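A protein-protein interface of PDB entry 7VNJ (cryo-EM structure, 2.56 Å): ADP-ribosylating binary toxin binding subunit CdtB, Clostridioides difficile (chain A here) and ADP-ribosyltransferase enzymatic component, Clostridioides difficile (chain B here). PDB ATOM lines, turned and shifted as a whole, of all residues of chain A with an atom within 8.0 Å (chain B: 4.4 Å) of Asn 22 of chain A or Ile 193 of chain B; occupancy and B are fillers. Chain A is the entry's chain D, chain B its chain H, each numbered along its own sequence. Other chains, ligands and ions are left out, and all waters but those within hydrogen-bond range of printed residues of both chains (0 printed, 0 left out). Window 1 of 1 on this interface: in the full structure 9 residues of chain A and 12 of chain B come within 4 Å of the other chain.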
ATOM      1  N   TRP A  13      -3.623 -12.066   7.740  1.00  0.00           N
ATOM      2  CA  TRP A  13      -2.403 -12.040   6.942  1.00  0.00           C
ATOM      3  C   TRP A  13      -1.130 -11.888   7.769  1.00  0.00           C
ATOM      4  O   TRP A  13      -1.106 -12.175   8.964  1.00  0.00           O
ATOM      5  CB  TRP A  13      -2.467 -10.915   5.917  1.00  0.00           C
ATOM      6  CG  TRP A  13      -2.754  -9.597   6.531  1.00  0.00           C
ATOM      7  CD1 TRP A  13      -1.882  -8.794   7.205  1.00  0.00           C
ATOM      8  CD2 TRP A  13      -3.992  -8.889   6.475  1.00  0.00           C
ATOM      9  NE1 TRP A  13      -2.514  -7.643   7.605  1.00  0.00           N
ATOM     10  CE2 TRP A  13      -3.810  -7.676   7.163  1.00  0.00           C
ATOM     11  CE3 TRP A  13      -5.242  -9.168   5.918  1.00  0.00           C
ATOM     12  CZ2 TRP A  13      -4.830  -6.745   7.311  1.00  0.00           C
ATOM     13  CZ3 TRP A  13      -6.249  -8.243   6.063  1.00  0.00           C
ATOM     14  CH2 TRP A  13      -6.041  -7.047   6.755  1.00  0.00           C
ATOM     15  N   ASP A  17      -1.643  -6.416  12.747  1.00  0.00           N
ATOM     16  CA  ASP A  17      -2.665  -5.382  12.669  1.00  0.00           C
ATOM     17  C   ASP A  17      -4.023  -6.009  12.392  1.00  0.00           C
ATOM     18  O   ASP A  17      -4.849  -5.461  11.658  1.00  0.00           O
ATOM     19  CB  ASP A  17      -2.317  -4.340  11.610  1.00  0.00           C
ATOM     20  CG  ASP A  17      -2.007  -4.956  10.261  1.00  0.00           C
ATOM     21  OD1 ASP A  17      -2.198  -6.179  10.097  1.00  0.00           O
ATOM     22  OD2 ASP A  17      -1.560  -4.214   9.362  1.00  0.00           O
ATOM     23  N   LEU A  18      -4.259  -7.182  12.969  1.00  0.00           N
ATOM     24  CA  LEU A  18      -5.524  -7.889  12.856  1.00  0.00           C
ATOM     25  C   LEU A  18      -6.212  -7.899  14.212  1.00  0.00           C
ATOM     26  O   LEU A  18      -5.611  -8.301  15.212  1.00  0.00           O
ATOM     27  CB  LEU A  18      -5.312  -9.324  12.374  1.00  0.00           C
ATOM     28  CG  LEU A  18      -4.918  -9.539  10.918  1.00  0.00           C
ATOM     29  CD1 LEU A  18      -4.637 -11.006  10.683  1.00  0.00           C
ATOM     30  CD2 LEU A  18      -6.013  -9.051   9.998  1.00  0.00           C
ATOM     31  N   ASP A  19      -7.465  -7.456  14.241  1.00  0.00           N
ATOM     32  CA  ASP A  19      -8.312  -7.538  15.430  1.00  0.00           C
ATOM     33  C   ASP A  19      -9.619  -8.179  14.983  1.00  0.00           C
ATOM     34  O   ASP A  19     -10.591  -7.487  14.680  1.00  0.00           O
ATOM     35  CB  ASP A  19      -8.527  -6.165  16.047  1.00  0.00           C
ATOM     36  CG  ASP A  19      -8.928  -6.238  17.501  1.00  0.00           C
ATOM     37  OD1 ASP A  19      -9.031  -7.359  18.034  1.00  0.00           O
ATOM     38  OD2 ASP A  19      -9.147  -5.173  18.109  1.00  0.00           O
ATOM     39  N   THR A  20      -9.638  -9.511  14.950  1.00  0.00           N
ATOM     40  CA  THR A  20     -10.783 -10.220  14.388  1.00  0.00           C
ATOM     41  C   THR A  20     -12.033 -10.031  15.238  1.00  0.00           C
ATOM     42  O   THR A  20     -13.127  -9.827  14.702  1.00  0.00           O
ATOM     43  CB  THR A  20     -10.456 -11.703  14.235  1.00  0.00           C
ATOM     44  OG1 THR A  20      -9.269 -11.850  13.448  1.00  0.00           O
ATOM     45  CG2 THR A  20     -11.593 -12.427  13.549  1.00  0.00           C
ATOM     46  N   ASP A  21     -11.897 -10.091  16.558  1.00  0.00           N
ATOM     47  CA  ASP A  21     -13.041  -9.953  17.446  1.00  0.00           C
ATOM     48  C   ASP A  21     -13.318  -8.510  17.840  1.00  0.00           C
ATOM     49  O   ASP A  21     -14.318  -8.254  18.518  1.00  0.00           O
ATOM     50  CB  ASP A  21     -12.840 -10.800  18.703  1.00  0.00           C
ATOM     51  CG  ASP A  21     -11.513 -10.543  19.366  1.00  0.00           C
ATOM     52  OD1 ASP A  21     -10.732  -9.735  18.832  1.00  0.00           O
ATOM     53  OD2 ASP A  21     -11.247 -11.147  20.423  1.00  0.00           O
ATOM     54  N   ASN A  22     -12.464  -7.572  17.435  1.00  0.00           N
ATOM     55  CA  ASN A  22     -12.662  -6.144  17.681  1.00  0.00           C
ATOM     56  C   ASN A  22     -12.750  -5.850  19.181  1.00  0.00           C
ATOM     57  O   ASN A  22     -13.756  -5.354  19.690  1.00  0.00           O
ATOM     58  CB  ASN A  22     -13.899  -5.632  16.937  1.00  0.00           C
ATOM     59  CG  ASN A  22     -14.006  -4.123  16.953  1.00  0.00           C
ATOM     60  OD1 ASN A  22     -13.001  -3.417  16.896  1.00  0.00           O
ATOM     61  ND2 ASN A  22     -15.231  -3.619  17.034  1.00  0.00           N
ATOM     62  N   ASP A  23     -11.667  -6.174  19.888  1.00  0.00           N
ATOM     63  CA  ASP A  23     -11.583  -5.927  21.323  1.00  0.00           C
ATOM     64  C   ASP A  23     -10.294  -5.206  21.704  1.00  0.00           C
ATOM     65  O   ASP A  23      -9.856  -5.306  22.853  1.00  0.00           O
ATOM     66  CB  ASP A  23     -11.716  -7.232  22.111  1.00  0.00           C
ATOM     67  CG  ASP A  23     -10.561  -8.184  21.876  1.00  0.00           C
ATOM     68  OD1 ASP A  23      -9.824  -8.011  20.885  1.00  0.00           O
ATOM     69  OD2 ASP A  23     -10.394  -9.119  22.684  1.00  0.00           O
ATOM     70  N   ASN A  24      -9.675  -4.500  20.757  1.00  0.00           N
ATOM     71  CA  ASN A  24      -8.499  -3.655  20.949  1.00  0.00           C
ATOM     72  C   ASN A  24      -7.226  -4.434  21.249  1.00  0.00           C
ATOM     73  O   ASN A  24      -6.230  -3.830  21.659  1.00  0.00           O
ATOM     74  CB  ASN A  24      -8.716  -2.614  22.054  1.00  0.00           C
ATOM     75  CG  ASN A  24      -9.942  -1.764  21.817  1.00  0.00           C
ATOM     76  OD1 ASN A  24     -10.172  -1.285  20.709  1.00  0.00           O
ATOM     77  ND2 ASN A  24     -10.737  -1.569  22.859  1.00  0.00           N
ATOM     78  N   ILE A  25      -7.219  -5.748  21.060  1.00  0.00           N
ATOM     79  CA  ILE A  25      -5.998  -6.530  21.230  1.00  0.00           C
ATOM     80  C   ILE A  25      -5.717  -7.287  19.937  1.00  0.00           C
ATOM     81  O   ILE A  25      -6.609  -7.968  19.416  1.00  0.00           O
ATOM     82  CB  ILE A  25      -6.100  -7.492  22.423  1.00  0.00           C
ATOM     83  CG1 ILE A  25      -6.685  -6.778  23.638  1.00  0.00           C
ATOM     84  CG2 ILE A  25      -4.734  -8.046  22.770  1.00  0.00           C
ATOM     85  CD1 ILE A  25      -7.133  -7.711  24.723  1.00  0.00           C
ATOM     86  N   ASP A  27      -4.565 -10.130  17.252  1.00  0.00           N
ATOM     87  CA  ASP A  27      -4.765 -11.575  17.316  1.00  0.00           C
ATOM     88  C   ASP A  27      -3.515 -12.290  17.813  1.00  0.00           C
ATOM     89  O   ASP A  27      -3.588 -13.158  18.690  1.00  0.00           O
ATOM     90  CB  ASP A  27      -5.171 -12.101  15.941  1.00  0.00           C
ATOM     91  CG  ASP A  27      -6.544 -11.628  15.522  1.00  0.00           C
ATOM     92  OD1 ASP A  27      -7.269 -11.076  16.373  1.00  0.00           O
ATOM     93  OD2 ASP A  27      -6.900 -11.809  14.340  1.00  0.00           O
ATOM     94  N   GLU A  30      -2.963 -11.893  21.607  1.00  0.00           N
ATOM     95  CA  GLU A  30      -3.768 -12.817  22.397  1.00  0.00           C
ATOM     96  C   GLU A  30      -3.277 -14.248  22.252  1.00  0.00           C
ATOM     97  O   GLU A  30      -3.409 -15.046  23.185  1.00  0.00           O
ATOM     98  CB  GLU A  30      -5.237 -12.730  21.990  1.00  0.00           C
ATOM     99  CG  GLU A  30      -5.866 -11.372  22.193  1.00  0.00           C
ATOM    100  CD  GLU A  30      -7.368 -11.394  22.032  1.00  0.00           C
ATOM    101  OE1 GLU A  30      -8.052 -11.987  22.886  1.00  0.00           O
ATOM    102  OE2 GLU A  30      -7.869 -10.819  21.047  1.00  0.00           O
ATOM    103  N   TYR A  60      -8.652 -15.135  20.658  1.00  0.00           N
ATOM    104  CA  TYR A  60      -8.599 -14.083  19.654  1.00  0.00           C
ATOM    105  C   TYR A  60      -9.821 -14.062  18.750  1.00  0.00           C
ATOM    106  O   TYR A  60      -9.978 -13.114  17.974  1.00  0.00           O
ATOM    107  CB  TYR A  60      -7.321 -14.213  18.819  1.00  0.00           C
ATOM    108  CG  TYR A  60      -7.359 -15.262  17.732  1.00  0.00           C
ATOM    109  CD1 TYR A  60      -7.072 -16.588  18.012  1.00  0.00           C
ATOM    110  CD2 TYR A  60      -7.654 -14.920  16.421  1.00  0.00           C
ATOM    111  CE1 TYR A  60      -7.095 -17.545  17.022  1.00  0.00           C
ATOM    112  CE2 TYR A  60      -7.681 -15.870  15.426  1.00  0.00           C
ATOM    113  CZ  TYR A  60      -7.400 -17.181  15.731  1.00  0.00           C
ATOM    114  OH  TYR A  60      -7.425 -18.132  14.742  1.00  0.00           O
ATOM    115  N   LEU A  61     -10.685 -15.069  18.830  1.00  0.00           N
ATOM    116  CA  LEU A  61     -11.944 -15.074  18.101  1.00  0.00           C
ATOM    117  C   LEU A  61     -13.134 -14.722  18.980  1.00  0.00           C
ATOM    118  O   LEU A  61     -14.268 -14.734  18.497  1.00  0.00           O
ATOM    119  CB  LEU A  61     -12.174 -16.441  17.451  1.00  0.00           C
ATOM    120  CG  LEU A  61     -11.278 -16.782  16.263  1.00  0.00           C
ATOM    121  CD1 LEU A  61     -11.706 -18.090  15.634  1.00  0.00           C
ATOM    122  CD2 LEU A  61     -11.307 -15.665  15.242  1.00  0.00           C
ATOM    123  N   GLU A  62     -12.904 -14.408  20.252  1.00  0.00           N
ATOM    124  CA  GLU A  62     -13.975 -14.128  21.197  1.00  0.00           C
ATOM    125  C   GLU A  62     -13.670 -12.837  21.937  1.00  0.00           C
ATOM    126  O   GLU A  62     -12.556 -12.653  22.435  1.00  0.00           O
ATOM    127  CB  GLU A  62     -14.141 -15.277  22.190  1.00  0.00           C
ATOM    128  CG  GLU A  62     -15.436 -15.232  22.959  1.00  0.00           C
ATOM    129  CD  GLU A  62     -16.629 -15.558  22.088  1.00  0.00           C
ATOM    130  OE1 GLU A  62     -16.529 -16.499  21.274  1.00  0.00           O
ATOM    131  OE2 GLU A  62     -17.665 -14.875  22.216  1.00  0.00           O
ATOM    132  N   SER A  63     -14.661 -11.949  22.012  1.00  0.00           N
ATOM    133  CA  SER A  63     -14.466 -10.686  22.714  1.00  0.00           C
ATOM    134  C   SER A  63     -14.463 -10.885  24.223  1.00  0.00           C
ATOM    135  O   SER A  63     -13.684 -10.246  24.938  1.00  0.00           O
ATOM    136  CB  SER A  63     -15.551  -9.692  22.307  1.00  0.00           C
ATOM    137  OG  SER A  63     -15.396  -8.467  22.994  1.00  0.00           O
ATOM    138  N   THR A  71     -15.158  -7.367  28.593  1.00  0.00           N
ATOM    139  CA  THR A  71     -14.321  -7.847  27.506  1.00  0.00           C
ATOM    140  C   THR A  71     -12.911  -8.155  28.006  1.00  0.00           C
ATOM    141  O   THR A  71     -12.548  -7.877  29.150  1.00  0.00           O
ATOM    142  CB  THR A  71     -14.263  -6.823  26.373  1.00  0.00           C
ATOM    143  OG1 THR A  71     -13.389  -5.749  26.737  1.00  0.00           O
ATOM    144  CG2 THR A  71     -15.642  -6.267  26.090  1.00  0.00           C
ATOM    145  N   TYR A  73     -10.070  -6.794  26.979  1.00  0.00           N
ATOM    146  CA  TYR A  73      -9.310  -5.572  27.214  1.00  0.00           C
ATOM    147  C   TYR A  73      -9.712  -4.908  28.523  1.00  0.00           C
ATOM    148  O   TYR A  73      -8.850  -4.439  29.274  1.00  0.00           O
ATOM    149  CB  TYR A  73      -9.491  -4.600  26.052  1.00  0.00           C
ATOM    150  CG  TYR A  73      -8.847  -3.260  26.305  1.00  0.00           C
ATOM    151  CD1 TYR A  73      -7.483  -3.085  26.132  1.00  0.00           C
ATOM    152  CD2 TYR A  73      -9.597  -2.176  26.733  1.00  0.00           C
ATOM    153  CE1 TYR A  73      -6.886  -1.867  26.369  1.00  0.00           C
ATOM    154  CE2 TYR A  73      -9.009  -0.955  26.975  1.00  0.00           C
ATOM    155  CZ  TYR A  73      -7.653  -0.806  26.790  1.00  0.00           C
ATOM    156  OH  TYR A  73      -7.061   0.410  27.027  1.00  0.00           O
ATOM    157  N   GLU B 143     -21.192   1.566  19.688  1.00  0.00           N
ATOM    158  CA  GLU B 143     -20.659   0.799  18.576  1.00  0.00           C
ATOM    159  C   GLU B 143     -21.796   0.263  17.706  1.00  0.00           C
ATOM    160  O   GLU B 143     -22.876  -0.061  18.208  1.00  0.00           O
ATOM    161  CB  GLU B 143     -19.800  -0.354  19.088  1.00  0.00           C
ATOM    162  CG  GLU B 143     -18.400   0.058  19.502  1.00  0.00           C
ATOM    163  CD  GLU B 143     -17.372  -1.017  19.216  1.00  0.00           C
ATOM    164  OE1 GLU B 143     -17.301  -1.994  19.990  1.00  0.00           O
ATOM    165  OE2 GLU B 143     -16.637  -0.886  18.215  1.00  0.00           O
ATOM    166  N   VAL B 191      -7.096  -1.420  11.415  1.00  0.00           N
ATOM    167  CA  VAL B 191      -7.079  -2.867  11.576  1.00  0.00           C
ATOM    168  C   VAL B 191      -8.294  -3.451  10.869  1.00  0.00           C
ATOM    169  O   VAL B 191      -9.282  -2.762  10.608  1.00  0.00           O
ATOM    170  CB  VAL B 191      -7.069  -3.297  13.059  1.00  0.00           C
ATOM    171  CG1 VAL B 191      -5.788  -2.847  13.740  1.00  0.00           C
ATOM    172  CG2 VAL B 191      -8.280  -2.739  13.780  1.00  0.00           C
ATOM    173  N   ARG B 192      -8.211  -4.742  10.562  1.00  0.00           N
ATOM    174  CA  ARG B 192      -9.315  -5.472   9.952  1.00  0.00           C
ATOM    175  C   ARG B 192     -10.091  -6.213  11.030  1.00  0.00           C
ATOM    176  O   ARG B 192      -9.510  -6.982  11.801  1.00  0.00           O
ATOM    177  CB  ARG B 192      -8.816  -6.458   8.896  1.00  0.00           C
ATOM    178  CG  ARG B 192      -9.942  -7.123   8.124  1.00  0.00           C
ATOM    179  CD  ARG B 192      -9.437  -8.221   7.209  1.00  0.00           C
ATOM    180  NE  ARG B 192      -9.048  -9.420   7.940  1.00  0.00           N
ATOM    181  CZ  ARG B 192      -8.564 -10.516   7.375  1.00  0.00           C
ATOM    182  NH1 ARG B 192      -8.403 -10.606   6.066  1.00  0.00           N
ATOM    183  NH2 ARG B 192      -8.234 -11.550   8.142  1.00  0.00           N
ATOM    184  N   ILE B 193     -11.401  -5.981  11.078  1.00  0.00           N
ATOM    185  CA  ILE B 193     -12.276  -6.594  12.066  1.00  0.00           C
ATOM    186  C   ILE B 193     -13.377  -7.360  11.341  1.00  0.00           C
ATOM    187  O   ILE B 193     -13.586  -7.207  10.139  1.00  0.00           O
ATOM    188  CB  ILE B 193     -12.879  -5.559  13.035  1.00  0.00           C
ATOM    189  CG1 ILE B 193     -13.995  -4.774  12.349  1.00  0.00           C
ATOM    190  CG2 ILE B 193     -11.807  -4.617  13.550  1.00  0.00           C
ATOM    191  CD1 ILE B 193     -14.784  -3.896  13.284  1.00  0.00           C
ATOM    192  N   VAL B 194     -14.083  -8.196  12.098  1.00  0.00           N
ATOM    193  CA  VAL B 194     -15.194  -8.990  11.587  1.00  0.00           C
ATOM    194  C   VAL B 194     -16.463  -8.554  12.303  1.00  0.00           C
ATOM    195  O   VAL B 194     -16.500  -8.513  13.538  1.00  0.00           O
ATOM    196  CB  VAL B 194     -14.957 -10.498  11.783  1.00  0.00           C
ATOM    197  CG1 VAL B 194     -16.219 -11.278  11.465  1.00  0.00           C
ATOM    198  CG2 VAL B 194     -13.806 -10.974  10.925  1.00  0.00           C
ATOM    199  N   ILE B 195     -17.497  -8.227  11.533  1.00  0.00           N
ATOM    200  CA  ILE B 195     -18.817  -7.916  12.068  1.00  0.00           C
ATOM    201  C   ILE B 195     -19.828  -8.785  11.332  1.00  0.00           C
ATOM    202  O   ILE B 195     -20.082  -8.572  10.141  1.00  0.00           O
ATOM    203  CB  ILE B 195     -19.176  -6.432  11.925  1.00  0.00           C
ATOM    204  CG1 ILE B 195     -18.156  -5.555  12.649  1.00  0.00           C
ATOM    205  CG2 ILE B 195     -20.570  -6.171  12.466  1.00  0.00           C
ATOM    206  CD1 ILE B 195     -18.380  -4.076  12.441  1.00  0.00           C
ATOM    207  N   LYS B 198     -18.573 -10.462   8.052  1.00  0.00           N
ATOM    208  CA  LYS B 198     -18.045  -9.620   6.992  1.00  0.00           C
ATOM    209  C   LYS B 198     -16.831  -8.864   7.509  1.00  0.00           C
ATOM    210  O   LYS B 198     -16.761  -8.501   8.685  1.00  0.00           O
ATOM    211  CB  LYS B 198     -19.094  -8.632   6.480  1.00  0.00           C
ATOM    212  CG  LYS B 198     -19.825  -9.096   5.239  1.00  0.00           C
ATOM    213  CD  LYS B 198     -20.687  -7.991   4.661  1.00  0.00           C
ATOM    214  CE  LYS B 198     -21.224  -8.378   3.297  1.00  0.00           C
ATOM    215  NZ  LYS B 198     -21.807  -7.213   2.581  1.00  0.00           N
ATOM    216  N   HIS B 199     -15.875  -8.628   6.617  1.00  0.00           N
ATOM    217  CA  HIS B 199     -14.669  -7.893   6.964  1.00  0.00           C
ATOM    218  C   HIS B 199     -14.890  -6.397   6.786  1.00  0.00           C
ATOM    219  O   HIS B 199     -15.473  -5.956   5.793  1.00  0.00           O
ATOM    220  CB  HIS B 199     -13.488  -8.350   6.106  1.00  0.00           C
ATOM    221  CG  HIS B 199     -12.825  -9.594   6.605  1.00  0.00           C
ATOM    222  ND1 HIS B 199     -12.167 -10.472   5.773  1.00  0.00           N
ATOM    223  CD2 HIS B 199     -12.720 -10.110   7.852  1.00  0.00           C
ATOM    224  CE1 HIS B 199     -11.687 -11.475   6.485  1.00  0.00           C
ATOM    225  NE2 HIS B 199     -12.008 -11.278   7.750  1.00  0.00           N
ATOM    226  N   TYR B 200     -14.420  -5.625   7.759  1.00  0.00           N
ATOM    227  CA  TYR B 200     -14.455  -4.172   7.710  1.00  0.00           C
ATOM    228  C   TYR B 200     -13.075  -3.638   8.061  1.00  0.00           C
ATOM    229  O   TYR B 200     -12.187  -4.378   8.486  1.00  0.00           O
ATOM    230  CB  TYR B 200     -15.502  -3.592   8.671  1.00  0.00           C
ATOM    231  CG  TYR B 200     -16.926  -3.984   8.359  1.00  0.00           C
ATOM    232  CD1 TYR B 200     -17.434  -5.208   8.769  1.00  0.00           C
ATOM    233  CD2 TYR B 200     -17.765  -3.126   7.664  1.00  0.00           C
ATOM    234  CE1 TYR B 200     -18.735  -5.568   8.489  1.00  0.00           C
ATOM    235  CE2 TYR B 200     -19.068  -3.479   7.381  1.00  0.00           C
ATOM    236  CZ  TYR B 200     -19.547  -4.701   7.796  1.00  0.00           C
ATOM    237  OH  TYR B 200     -20.844  -5.063   7.519  1.00  0.00           O
ATOM    238  N   LYS B 202     -11.451  -0.743  10.511  1.00  0.00           N
ATOM    239  CA  LYS B 202     -11.703   0.155  11.629  1.00  0.00           C
ATOM    240  C   LYS B 202     -10.518   1.097  11.765  1.00  0.00           C
ATOM    241  O   LYS B 202      -9.375   0.647  11.899  1.00  0.00           O
ATOM    242  CB  LYS B 202     -11.927  -0.630  12.920  1.00  0.00           C
ATOM    243  CG  LYS B 202     -12.490   0.195  14.061  1.00  0.00           C
ATOM    244  CD  LYS B 202     -11.433   0.492  15.105  1.00  0.00           C
ATOM    245  CE  LYS B 202     -11.119  -0.740  15.930  1.00  0.00           C
ATOM    246  NZ  LYS B 202     -10.132  -0.446  17.004  1.00  0.00           N
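O of Arg 192 of chain B lies within hydrogen-bond range of N of Asp 19 of chain A (3.2 Å).
The backbone NH (N) of Val 194 of chain B lies within hydrogen-bond range of the backbone carbonyl oxygen (O) of Thr 20 of chain A, at 3.2 Å.
OE2 of Glu 143 of chain B is in hydrogen-bond range of ND2 of Asn 22 of chain A (3.3 Å).
OD1 of Asp 17 of chain A is in hydrogen-bond range of NE1 of Trp 13 of chain A (2.9 Å).
N of Asp 27 of chain A lies within hydrogen-bond range of O of Leu 18 of chain A.
OD1 of Asp 19 of chain A sits close to N of Asn 22 of chain A (3.5 Å).
OD2 of Asp 27 of chain A lies within hydrogen-bond range of OG1 of Thr 20 of chain A, 2.5 Å away.
The backbone carbonyl oxygen of Val 191 of chain B sits at hydrogen-bond distance from the backbone NH of Lys 202 of chain B, at 3.0 Å.
N of Tyr 200 of chain B lies within hydrogen-bond range of O of Ile 193 of chain B.
Among the printed residues, merely in contact across the chains: Trp 13 of chain A with Arg 192 of chain B (3.2 Å), Asp 17 of chain A with Val 191 of chain B (3.4 Å), Asp 17 of chain A with Arg 192 of chain B (3.6 Å), Leu 18 of chain A with Arg 192 of chain B (3.7 Å), Asp 19 of chain A with Ile 193 of chain B (3.2 Å), Asn 22 of chain A with Ile 193 of chain B (3.7 Å), Asn 22 of chain A with Lys 202 of chain B (3.4 Å) and Asn 24 of chain A with Lys 202 of chain B (3.8 Å).
Printed residues of chain B within 4 Å of Trp 13 of chain A: Arg 192 (3.2 Å).
Of the printed residues of chain B, Asp 17 of chain A touches Val 191 (3.4 Å) and Arg 192 (3.6 Å).
Of the printed residues of chain B, Leu 18 of chain A touches Arg 192.
Of the printed residues of chain B, Asn 22 of chain A touches Glu 143 (3.3 Å), Ile 193 (3.7 Å) and Lys 202 (3.4 Å).
Ser 63 of chain A touches none of the printed residues of chain B.
Of the printed residues of chain A, Arg 192 of chain B touches Trp 13 (3.2 Å), Asp 17 (3.6 Å), Leu 18 (3.7 Å) and Asp 19 (3.1 Å).
Ile 193 of chain B touches just these residues of chain A: Asp 19 (3.2 Å) and Asn 22 (3.7 Å).
Of the printed residues of chain A, Val 194 of chain B touches Thr 20 (3.2 Å).
The nearest residue of chain A that does not touch Ile 193 of chain B is Thr 20 of chain A (4.2 Å).
Among the printed residues, no Asp or Glu carboxylate lies within 4 Å of a Lys or Arg side-chain nitrogen of the other chain.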
